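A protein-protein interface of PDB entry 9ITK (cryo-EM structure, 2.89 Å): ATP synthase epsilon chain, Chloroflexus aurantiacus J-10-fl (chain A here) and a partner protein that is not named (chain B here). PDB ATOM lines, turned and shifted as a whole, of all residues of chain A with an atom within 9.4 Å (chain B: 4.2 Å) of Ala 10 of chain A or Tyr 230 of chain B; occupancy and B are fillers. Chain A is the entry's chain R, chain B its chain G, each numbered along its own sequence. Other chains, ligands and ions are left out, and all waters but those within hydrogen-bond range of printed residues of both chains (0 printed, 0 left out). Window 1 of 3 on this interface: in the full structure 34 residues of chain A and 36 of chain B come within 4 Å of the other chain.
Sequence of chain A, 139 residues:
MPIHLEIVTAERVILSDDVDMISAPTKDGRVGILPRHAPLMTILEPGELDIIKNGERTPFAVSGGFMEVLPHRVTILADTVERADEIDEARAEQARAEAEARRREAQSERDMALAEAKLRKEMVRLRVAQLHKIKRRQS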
ATOM      1  N   ILE A   7       2.384 -36.206  -0.650  1.00  0.00           N
ATOM      2  CA  ILE A   7       1.511 -35.367   0.170  1.00  0.00           C
ATOM      3  C   ILE A   7       0.770 -34.438  -0.785  1.00  0.00           C
ATOM      4  O   ILE A   7       1.312 -33.425  -1.228  1.00  0.00           O
ATOM      5  CB  ILE A   7       2.278 -34.582   1.236  1.00  0.00           C
ATOM      6  CG1 ILE A   7       2.957 -35.516   2.236  1.00  0.00           C
ATOM      7  CG2 ILE A   7       1.343 -33.637   1.970  1.00  0.00           C
ATOM      8  CD1 ILE A   7       4.347 -35.913   1.850  1.00  0.00           C
ATOM      9  N   VAL A   8      -0.471 -34.779  -1.107  1.00  0.00           N
ATOM     10  CA  VAL A   8      -1.271 -34.026  -2.063  1.00  0.00           C
ATOM     11  C   VAL A   8      -2.316 -33.227  -1.301  1.00  0.00           C
ATOM     12  O   VAL A   8      -3.048 -33.780  -0.473  1.00  0.00           O
ATOM     13  CB  VAL A   8      -1.932 -34.959  -3.089  1.00  0.00           C
ATOM     14  CG1 VAL A   8      -2.870 -34.177  -3.983  1.00  0.00           C
ATOM     15  CG2 VAL A   8      -0.875 -35.669  -3.912  1.00  0.00           C
ATOM     16  N   THR A   9      -2.385 -31.932  -1.579  1.00  0.00           N
ATOM     17  CA  THR A   9      -3.371 -31.047  -0.984  1.00  0.00           C
ATOM     18  C   THR A   9      -4.313 -30.559  -2.076  1.00  0.00           C
ATOM     19  O   THR A   9      -3.954 -30.531  -3.256  1.00  0.00           O
ATOM     20  CB  THR A   9      -2.701 -29.854  -0.285  1.00  0.00           C
ATOM     21  OG1 THR A   9      -1.573 -30.315   0.467  1.00  0.00           O
ATOM     22  CG2 THR A   9      -3.670 -29.162   0.661  1.00  0.00           C
ATOM     23  N   ALA A  10      -5.531 -30.188  -1.674  1.00  0.00           N
ATOM     24  CA  ALA A  10      -6.517 -29.709  -2.635  1.00  0.00           C
ATOM     25  C   ALA A  10      -6.044 -28.472  -3.383  1.00  0.00           C
ATOM     26  O   ALA A  10      -6.560 -28.182  -4.468  1.00  0.00           O
ATOM     27  CB  ALA A  10      -7.838 -29.414  -1.928  1.00  0.00           C
ATOM     28  N   GLU A  11      -5.084 -27.734  -2.831  1.00  0.00           N
ATOM     29  CA  GLU A  11      -4.530 -26.569  -3.510  1.00  0.00           C
ATOM     30  C   GLU A  11      -3.367 -26.940  -4.423  1.00  0.00           C
ATOM     31  O   GLU A  11      -3.353 -26.560  -5.598  1.00  0.00           O
ATOM     32  CB  GLU A  11      -4.085 -25.528  -2.480  1.00  0.00           C
ATOM     33  CG  GLU A  11      -5.206 -24.632  -1.985  1.00  0.00           C
ATOM     34  CD  GLU A  11      -6.059 -25.302  -0.929  1.00  0.00           C
ATOM     35  OE1 GLU A  11      -5.652 -26.368  -0.423  1.00  0.00           O
ATOM     36  OE2 GLU A  11      -7.137 -24.763  -0.603  1.00  0.00           O
ATOM     37  N   ARG A  12      -2.393 -27.686  -3.906  1.00  0.00           N
ATOM     38  CA  ARG A  12      -1.203 -28.009  -4.681  1.00  0.00           C
ATOM     39  C   ARG A  12      -0.541 -29.247  -4.097  1.00  0.00           C
ATOM     40  O   ARG A  12      -0.759 -29.604  -2.938  1.00  0.00           O
ATOM     41  CB  ARG A  12      -0.221 -26.835  -4.700  1.00  0.00           C
ATOM     42  CG  ARG A  12       0.288 -26.450  -3.323  1.00  0.00           C
ATOM     43  CD  ARG A  12       1.373 -25.393  -3.403  1.00  0.00           C
ATOM     44  NE  ARG A  12       2.282 -25.472  -2.266  1.00  0.00           N
ATOM     45  CZ  ARG A  12       3.405 -26.177  -2.253  1.00  0.00           C
ATOM     46  NH1 ARG A  12       3.795 -26.874  -3.307  1.00  0.00           N
ATOM     47  NH2 ARG A  12       4.155 -26.183  -1.154  1.00  0.00           N
ATOM     48  N   VAL A  13       0.283 -29.889  -4.919  1.00  0.00           N
ATOM     49  CA  VAL A  13       1.054 -31.048  -4.483  1.00  0.00           C
ATOM     50  C   VAL A  13       2.253 -30.564  -3.681  1.00  0.00           C
ATOM     51  O   VAL A  13       2.974 -29.656  -4.109  1.00  0.00           O
ATOM     52  CB  VAL A  13       1.495 -31.891  -5.690  1.00  0.00           C
ATOM     53  CG1 VAL A  13       2.462 -32.978  -5.254  1.00  0.00           C
ATOM     54  CG2 VAL A  13       0.286 -32.493  -6.383  1.00  0.00           C
ATOM     55  N   ILE A  14       2.468 -31.167  -2.513  1.00  0.00           N
ATOM     56  CA  ILE A  14       3.521 -30.716  -1.608  1.00  0.00           C
ATOM     57  C   ILE A  14       4.799 -31.509  -1.843  1.00  0.00           C
ATOM     58  O   ILE A  14       5.868 -30.928  -2.067  1.00  0.00           O
ATOM     59  CB  ILE A  14       3.068 -30.821  -0.142  1.00  0.00           C
ATOM     60  CG1 ILE A  14       1.621 -30.352  -0.005  1.00  0.00           C
ATOM     61  CG2 ILE A  14       3.968 -29.987   0.747  1.00  0.00           C
ATOM     62  CD1 ILE A  14       1.413 -28.900  -0.364  1.00  0.00           C
ATOM     63  N   GLY A  64      -5.881 -32.411   9.414  1.00  0.00           N
ATOM     64  CA  GLY A  64      -6.863 -33.384   8.989  1.00  0.00           C
ATOM     65  C   GLY A  64      -6.609 -33.812   7.566  1.00  0.00           C
ATOM     66  O   GLY A  64      -5.895 -33.160   6.805  1.00  0.00           O
ATOM     67  N   GLY A  65      -7.206 -34.932   7.204  1.00  0.00           N
ATOM     68  CA  GLY A  65      -7.065 -35.459   5.867  1.00  0.00           C
ATOM     69  C   GLY A  65      -7.199 -36.967   5.873  1.00  0.00           C
ATOM     70  O   GLY A  65      -7.601 -37.569   6.863  1.00  0.00           O
ATOM     71  N   ILE A  76      -1.187 -39.012   0.604  1.00  0.00           N
ATOM     72  CA  ILE A  76      -1.754 -38.322   1.756  1.00  0.00           C
ATOM     73  C   ILE A  76      -2.570 -37.154   1.222  1.00  0.00           C
ATOM     74  O   ILE A  76      -2.020 -36.099   0.888  1.00  0.00           O
ATOM     75  CB  ILE A  76      -0.680 -37.849   2.740  1.00  0.00           C
ATOM     76  CG1 ILE A  76       0.080 -39.048   3.302  1.00  0.00           C
ATOM     77  CG2 ILE A  76      -1.305 -37.044   3.865  1.00  0.00           C
ATOM     78  CD1 ILE A  76       1.293 -38.671   4.108  1.00  0.00           C
ATOM     79  N   LEU A  77      -3.885 -37.333   1.146  1.00  0.00           N
ATOM     80  CA  LEU A  77      -4.775 -36.273   0.694  1.00  0.00           C
ATOM     81  C   LEU A  77      -5.119 -35.351   1.855  1.00  0.00           C
ATOM     82  O   LEU A  77      -6.297 -35.126   2.148  1.00  0.00           O
ATOM     83  CB  LEU A  77      -6.045 -36.870   0.090  1.00  0.00           C
ATOM     84  CG  LEU A  77      -5.802 -37.969  -0.939  1.00  0.00           C
ATOM     85  CD1 LEU A  77      -7.113 -38.545  -1.423  1.00  0.00           C
ATOM     86  CD2 LEU A  77      -5.004 -37.418  -2.099  1.00  0.00           C
ATOM     87  N   ALA A  78      -4.081 -34.857   2.539  1.00  0.00           N
ATOM     88  CA  ALA A  78      -4.295 -33.987   3.720  1.00  0.00           C
ATOM     89  C   ALA A  78      -5.010 -32.702   3.297  1.00  0.00           C
ATOM     90  O   ALA A  78      -4.613 -32.112   2.272  1.00  0.00           O
ATOM     91  CB  ALA A  78      -2.973 -33.688   4.383  1.00  0.00           C
ATOM     92  N   ASP A  79      -6.023 -32.291   4.062  1.00  0.00           N
ATOM     93  CA  ASP A  79      -6.775 -31.048   3.745  1.00  0.00           C
ATOM     94  C   ASP A  79      -5.858 -29.836   3.940  1.00  0.00           C
ATOM     95  O   ASP A  79      -5.897 -28.931   3.085  1.00  0.00           O
ATOM     96  CB  ASP A  79      -8.051 -30.946   4.584  1.00  0.00           C
ATOM     97  CG  ASP A  79      -8.998 -32.116   4.376  1.00  0.00           C
ATOM     98  OD1 ASP A  79      -8.640 -33.031   3.608  1.00  0.00           O
ATOM     99  OD2 ASP A  79     -10.086 -32.101   4.984  1.00  0.00           O
ATOM    100  N   THR A  80      -5.065 -29.823   5.019  1.00  0.00           N
ATOM    101  CA  THR A  80      -4.202 -28.646   5.316  1.00  0.00           C
ATOM    102  C   THR A  80      -2.879 -29.089   5.949  1.00  0.00           C
ATOM    103  O   THR A  80      -2.876 -30.126   6.640  1.00  0.00           O
ATOM    104  CB  THR A  80      -4.913 -27.660   6.251  1.00  0.00           C
ATOM    105  OG1 THR A  80      -5.185 -28.342   7.475  1.00  0.00           O
ATOM    106  CG2 THR A  80      -6.197 -27.110   5.672  1.00  0.00           C
ATOM    107  N   VAL A  81      -1.805 -28.322   5.728  1.00  0.00           N
ATOM    108  CA  VAL A  81      -0.485 -28.624   6.359  1.00  0.00           C
ATOM    109  C   VAL A  81       0.017 -27.338   7.024  1.00  0.00           C
ATOM    110  O   VAL A  81      -0.239 -26.257   6.460  1.00  0.00           O
ATOM    111  CB  VAL A  81       0.529 -29.169   5.334  1.00  0.00           C
ATOM    112  CG1 VAL A  81       1.887 -29.429   5.968  1.00  0.00           C
ATOM    113  CG2 VAL A  81       0.012 -30.421   4.642  1.00  0.00           C
ATOM    114  N   ARG A 102       0.323 -13.950  -5.349  1.00  0.00           N
ATOM    115  CA  ARG A 102      -0.984 -14.365  -5.925  1.00  0.00           C
ATOM    116  C   ARG A 102      -2.024 -13.287  -5.601  1.00  0.00           C
ATOM    117  O   ARG A 102      -3.198 -13.648  -5.382  1.00  0.00           O
ATOM    118  CB  ARG A 102      -1.403 -15.728  -5.366  1.00  0.00           C
ATOM    119  CG  ARG A 102      -0.478 -16.869  -5.763  1.00  0.00           C
ATOM    120  CD  ARG A 102      -0.478 -17.097  -7.263  1.00  0.00           C
ATOM    121  NE  ARG A 102      -1.790 -17.484  -7.761  1.00  0.00           N
ATOM    122  CZ  ARG A 102      -2.058 -17.777  -9.028  1.00  0.00           C
ATOM    123  NH1 ARG A 102      -1.098 -17.732  -9.936  1.00  0.00           N
ATOM    124  NH2 ARG A 102      -3.284 -18.119  -9.384  1.00  0.00           N
ATOM    125  N   THR B  42      -4.801 -28.697  -9.320  1.00  0.00           N
ATOM    126  CA  THR B  42      -5.806 -29.398  -8.532  1.00  0.00           C
ATOM    127  C   THR B  42      -6.164 -30.757  -9.121  1.00  0.00           C
ATOM    128  O   THR B  42      -6.811 -31.562  -8.442  1.00  0.00           O
ATOM    129  CB  THR B  42      -7.062 -28.531  -8.411  1.00  0.00           C
ATOM    130  OG1 THR B  42      -6.678 -27.173  -8.167  1.00  0.00           O
ATOM    131  CG2 THR B  42      -7.946 -29.000  -7.265  1.00  0.00           C
ATOM    132  N   TYR B  45      -5.232 -34.092  -7.068  1.00  0.00           N
ATOM    133  CA  TYR B  45      -6.031 -34.277  -5.861  1.00  0.00           C
ATOM    134  C   TYR B  45      -7.422 -34.795  -6.196  1.00  0.00           C
ATOM    135  O   TYR B  45      -7.909 -35.745  -5.575  1.00  0.00           O
ATOM    136  CB  TYR B  45      -6.116 -32.961  -5.092  1.00  0.00           C
ATOM    137  CG  TYR B  45      -6.800 -33.064  -3.750  1.00  0.00           C
ATOM    138  CD1 TYR B  45      -8.174 -32.914  -3.637  1.00  0.00           C
ATOM    139  CD2 TYR B  45      -6.071 -33.297  -2.595  1.00  0.00           C
ATOM    140  CE1 TYR B  45      -8.800 -32.997  -2.414  1.00  0.00           C
ATOM    141  CE2 TYR B  45      -6.691 -33.382  -1.366  1.00  0.00           C
ATOM    142  CZ  TYR B  45      -8.056 -33.232  -1.282  1.00  0.00           C
ATOM    143  OH  TYR B  45      -8.679 -33.318  -0.060  1.00  0.00           O
ATOM    144  N   PRO B 147      -9.152 -18.872  -5.772  1.00  0.00           N
ATOM    145  CA  PRO B 147      -9.707 -19.165  -4.450  1.00  0.00           C
ATOM    146  C   PRO B 147      -9.212 -20.499  -3.914  1.00  0.00           C
ATOM    147  O   PRO B 147      -8.786 -21.386  -4.656  1.00  0.00           O
ATOM    148  CB  PRO B 147     -11.216 -19.203  -4.706  1.00  0.00           C
ATOM    149  CG  PRO B 147     -11.325 -19.678  -6.109  1.00  0.00           C
ATOM    150  CD  PRO B 147     -10.129 -19.129  -6.846  1.00  0.00           C
ATOM    151  N   LYS B 148      -9.276 -20.626  -2.595  1.00  0.00           N
ATOM    152  CA  LYS B 148      -8.955 -21.870  -1.914  1.00  0.00           C
ATOM    153  C   LYS B 148     -10.236 -22.621  -1.569  1.00  0.00           C
ATOM    154  O   LYS B 148     -11.326 -22.048  -1.520  1.00  0.00           O
ATOM    155  CB  LYS B 148      -8.139 -21.605  -0.648  1.00  0.00           C
ATOM    156  CG  LYS B 148      -6.750 -21.053  -0.919  1.00  0.00           C
ATOM    157  CD  LYS B 148      -5.998 -20.794   0.374  1.00  0.00           C
ATOM    158  CE  LYS B 148      -6.757 -19.825   1.261  1.00  0.00           C
ATOM    159  NZ  LYS B 148      -7.052 -18.550   0.554  1.00  0.00           N
ATOM    160  N   LEU B 149     -10.089 -23.927  -1.332  1.00  0.00           N
ATOM    161  CA  LEU B 149     -11.250 -24.764  -1.057  1.00  0.00           C
ATOM    162  C   LEU B 149     -11.958 -24.356   0.228  1.00  0.00           C
ATOM    163  O   LEU B 149     -13.152 -24.635   0.379  1.00  0.00           O
ATOM    164  CB  LEU B 149     -10.825 -26.237  -1.021  1.00  0.00           C
ATOM    165  CG  LEU B 149     -11.873 -27.351  -0.924  1.00  0.00           C
ATOM    166  CD1 LEU B 149     -11.335 -28.620  -1.548  1.00  0.00           C
ATOM    167  CD2 LEU B 149     -12.234 -27.636   0.517  1.00  0.00           C
ATOM    168  N   ILE B 152     -15.183 -22.156  -0.442  1.00  0.00           N
ATOM    169  CA  ILE B 152     -16.439 -22.768  -0.872  1.00  0.00           C
ATOM    170  C   ILE B 152     -17.086 -23.623   0.203  1.00  0.00           C
ATOM    171  O   ILE B 152     -18.194 -24.130  -0.009  1.00  0.00           O
ATOM    172  CB  ILE B 152     -16.226 -23.620  -2.138  1.00  0.00           C
ATOM    173  CG1 ILE B 152     -15.643 -24.983  -1.771  1.00  0.00           C
ATOM    174  CG2 ILE B 152     -15.311 -22.902  -3.110  1.00  0.00           C
ATOM    175  CD1 ILE B 152     -15.780 -26.011  -2.862  1.00  0.00           C
ATOM    176  N   GLU B 226     -17.036 -31.723  -2.057  1.00  0.00           N
ATOM    177  CA  GLU B 226     -16.389 -30.418  -1.998  1.00  0.00           C
ATOM    178  C   GLU B 226     -15.338 -30.283  -3.091  1.00  0.00           C
ATOM    179  O   GLU B 226     -15.183 -29.211  -3.685  1.00  0.00           O
ATOM    180  CB  GLU B 226     -15.762 -30.199  -0.623  1.00  0.00           C
ATOM    181  CG  GLU B 226     -16.756 -29.828   0.459  1.00  0.00           C
ATOM    182  CD  GLU B 226     -16.268 -30.198   1.844  1.00  0.00           C
ATOM    183  OE1 GLU B 226     -15.164 -30.772   1.952  1.00  0.00           O
ATOM    184  OE2 GLU B 226     -16.986 -29.915   2.824  1.00  0.00           O
ATOM    185  N   THR B 227     -14.601 -31.361  -3.364  1.00  0.00           N
ATOM    186  CA  THR B 227     -13.625 -31.333  -4.446  1.00  0.00           C
ATOM    187  C   THR B 227     -14.302 -31.133  -5.796  1.00  0.00           C
ATOM    188  O   THR B 227     -13.799 -30.387  -6.644  1.00  0.00           O
ATOM    189  CB  THR B 227     -12.802 -32.618  -4.441  1.00  0.00           C
ATOM    190  OG1 THR B 227     -12.105 -32.731  -3.196  1.00  0.00           O
ATOM    191  CG2 THR B 227     -11.794 -32.608  -5.572  1.00  0.00           C
ATOM    192  N   GLN B 228     -15.444 -31.787  -6.016  1.00  0.00           N
ATOM    193  CA  GLN B 228     -16.173 -31.587  -7.265  1.00  0.00           C
ATOM    194  C   GLN B 228     -16.624 -30.140  -7.415  1.00  0.00           C
ATOM    195  O   GLN B 228     -16.513 -29.557  -8.500  1.00  0.00           O
ATOM    196  CB  GLN B 228     -17.376 -32.523  -7.335  1.00  0.00           C
ATOM    197  CG  GLN B 228     -17.040 -33.991  -7.223  1.00  0.00           C
ATOM    198  CD  GLN B 228     -18.101 -34.869  -7.850  1.00  0.00           C
ATOM    199  OE1 GLN B 228     -18.946 -35.433  -7.157  1.00  0.00           O
ATOM    200  NE2 GLN B 228     -18.066 -34.986  -9.171  1.00  0.00           N
ATOM    201  N   ILE B 229     -17.140 -29.546  -6.337  1.00  0.00           N
ATOM    202  CA  ILE B 229     -17.538 -28.142  -6.387  1.00  0.00           C
ATOM    203  C   ILE B 229     -16.321 -27.256  -6.612  1.00  0.00           C
ATOM    204  O   ILE B 229     -16.350 -26.330  -7.432  1.00  0.00           O
ATOM    205  CB  ILE B 229     -18.293 -27.753  -5.105  1.00  0.00           C
ATOM    206  CG1 ILE B 229     -19.581 -28.563  -4.979  1.00  0.00           C
ATOM    207  CG2 ILE B 229     -18.610 -26.272  -5.104  1.00  0.00           C
ATOM    208  CD1 ILE B 229     -20.401 -28.210  -3.761  1.00  0.00           C
ATOM    209  N   TYR B 230     -15.230 -27.528  -5.895  1.00  0.00           N
ATOM    210  CA  TYR B 230     -14.015 -26.743  -6.071  1.00  0.00           C
ATOM    211  C   TYR B 230     -13.466 -26.884  -7.483  1.00  0.00           C
ATOM    212  O   TYR B 230     -12.994 -25.907  -8.075  1.00  0.00           O
ATOM    213  CB  TYR B 230     -12.965 -27.166  -5.048  1.00  0.00           C
ATOM    214  CG  TYR B 230     -11.781 -26.240  -4.970  1.00  0.00           C
ATOM    215  CD1 TYR B 230     -11.929 -24.932  -4.542  1.00  0.00           C
ATOM    216  CD2 TYR B 230     -10.511 -26.676  -5.315  1.00  0.00           C
ATOM    217  CE1 TYR B 230     -10.848 -24.081  -4.466  1.00  0.00           C
ATOM    218  CE2 TYR B 230      -9.423 -25.832  -5.239  1.00  0.00           C
ATOM    219  CZ  TYR B 230      -9.598 -24.536  -4.812  1.00  0.00           C
ATOM    220  OH  TYR B 230      -8.520 -23.686  -4.735  1.00  0.00           O
ATOM    221  N   GLN B 231     -13.508 -28.095  -8.037  1.00  0.00           N
ATOM    222  CA  GLN B 231     -13.050 -28.294  -9.406  1.00  0.00           C
ATOM    223  C   GLN B 231     -13.927 -27.536 -10.393  1.00  0.00           C
ATOM    224  O   GLN B 231     -13.427 -26.969 -11.371  1.00  0.00           O
ATOM    225  CB  GLN B 231     -13.024 -29.784  -9.739  1.00  0.00           C
ATOM    226  CG  GLN B 231     -12.014 -30.165 -10.803  1.00  0.00           C
ATOM    227  CD  GLN B 231     -10.596 -30.187 -10.270  1.00  0.00           C
ATOM    228  OE1 GLN B 231     -10.372 -30.436  -9.087  1.00  0.00           O
ATOM    229  NE2 GLN B 231      -9.631 -29.929 -11.143  1.00  0.00           N
ATOM    230  N   ALA B 232     -15.241 -27.521 -10.158  1.00  0.00           N
ATOM    231  CA  ALA B 232     -16.137 -26.769 -11.030  1.00  0.00           C
ATOM    232  C   ALA B 232     -15.902 -25.268 -10.909  1.00  0.00           C
ATOM    233  O   ALA B 232     -15.948 -24.546 -11.911  1.00  0.00           O
ATOM    234  CB  ALA B 232     -17.591 -27.111 -10.715  1.00  0.00           C
ATOM    235  N   VAL B 233     -15.657 -24.780  -9.692  1.00  0.00           N
ATOM    236  CA  VAL B 233     -15.408 -23.354  -9.502  1.00  0.00           C
ATOM    237  C   VAL B 233     -14.129 -22.934 -10.216  1.00  0.00           C
ATOM    238  O   VAL B 233     -14.100 -21.924 -10.927  1.00  0.00           O
ATOM    239  CB  VAL B 233     -15.353 -23.013  -8.003  1.00  0.00           C
ATOM    240  CG1 VAL B 233     -14.775 -21.628  -7.796  1.00  0.00           C
ATOM    241  CG2 VAL B 233     -16.739 -23.096  -7.399  1.00  0.00           C
ATOM    242  N   LEU B 234     -13.056 -23.707 -10.045  1.00  0.00           N
ATOM    243  CA  LEU B 234     -11.797 -23.371 -10.704  1.00  0.00           C
ATOM    244  C   LEU B 234     -11.923 -23.466 -12.218  1.00  0.00           C
ATOM    245  O   LEU B 234     -11.362 -22.641 -12.947  1.00  0.00           O
ATOM    246  CB  LEU B 234     -10.677 -24.277 -10.198  1.00  0.00           C
ATOM    247  CG  LEU B 234      -9.822 -23.704  -9.069  1.00  0.00           C
ATOM    248  CD1 LEU B 234      -9.035 -22.507  -9.567  1.00  0.00           C
ATOM    249  CD2 LEU B 234     -10.681 -23.312  -7.885  1.00  0.00           C
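The backbone NH (N) of Leu 149 of chain B lies within hydrogen-bond range of the side-chain carboxylate (OE2) of Glu 11 of chain A (3.2 Å).
Tyr 45 of chain B touches Val 8 of chain A.
Thr 9 of chain A touches Tyr 45 of chain B.
O of Ala 10 of chain A touches CG2 of Thr 42 of chain B, at 3.2 Å.
Ala 10 of chain A touches Tyr 45 of chain B.
CD1 of Leu 149 of chain B touches CB of Ala 10 of chain A (3.6 Å).
Ala 10 of chain A touches Tyr 230 of chain B (O to CE2, 3.8 Å).
OE2 of Glu 11 of chain A touches CB of Lys 148 of chain B (3.3 Å).
Leu 77 of chain A touches Tyr 45 of chain B (O to OH, 3.7 Å).
Asp 79 of chain A touches Tyr 45 of chain B.
Hydrophobic or aromatic side chains of chain A within 4 Å of the printed part of chain B: Val 8, Ala 10 and Leu 77.
Along chain A the printed residues that touch a printed residue of chain B span positions 8 to 79.
Hydrophobic or aromatic side chains of chain B that line the printed part of chain A: Tyr 45, Leu 149 and Tyr 230.
Printed residues of chain B within 4 Å of Val 8 of chain A: Tyr 45.
Of the printed residues of chain B, Ala 10 of chain A touches Thr 42 (3.2 Å), Tyr 45 (3.3 Å), Leu 149 (3.6 Å) and Tyr 230 (3.8 Å).
Of the printed residues of chain B, Glu 11 of chain A touches Lys 148 (3.3 Å) and Leu 149 (3.2 Å).
Of the printed residues of chain B, Asp 79 of chain A touches Tyr 45.
Of chain A, only Ala 10 (3.2 Å) comes within 4 Å of Thr 42 of chain B.
No residue of chain A comes within 4 Å of Pro 147 of chain B.
Printed residues of chain A within 4 Å of Tyr 230 of chain B: Ala 10 (3.8 Å).
No residue of chain A comes within 4 Å of Val 233 of chain B.
The nearest residue of chain A that does not touch Tyr 230 of chain B is Glu 11 of chain A (4.4 Å).
The nearest printed residue of chain B that does not touch Leu 77 of chain A is Thr 227 of chain B (7.9 Å).
The backbone NH of Asp 79 of chain A sits at hydrogen-bond distance from the backbone carbonyl oxygen of Gly 64 of chain A, 2.9 Å away.
O of Ile 76 of chain A lies within hydrogen-bond range of N of Val 8 of chain A (2.8 Å).
O of Val 8 of chain A lies within hydrogen-bond range of N of Ala 78 of chain A.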
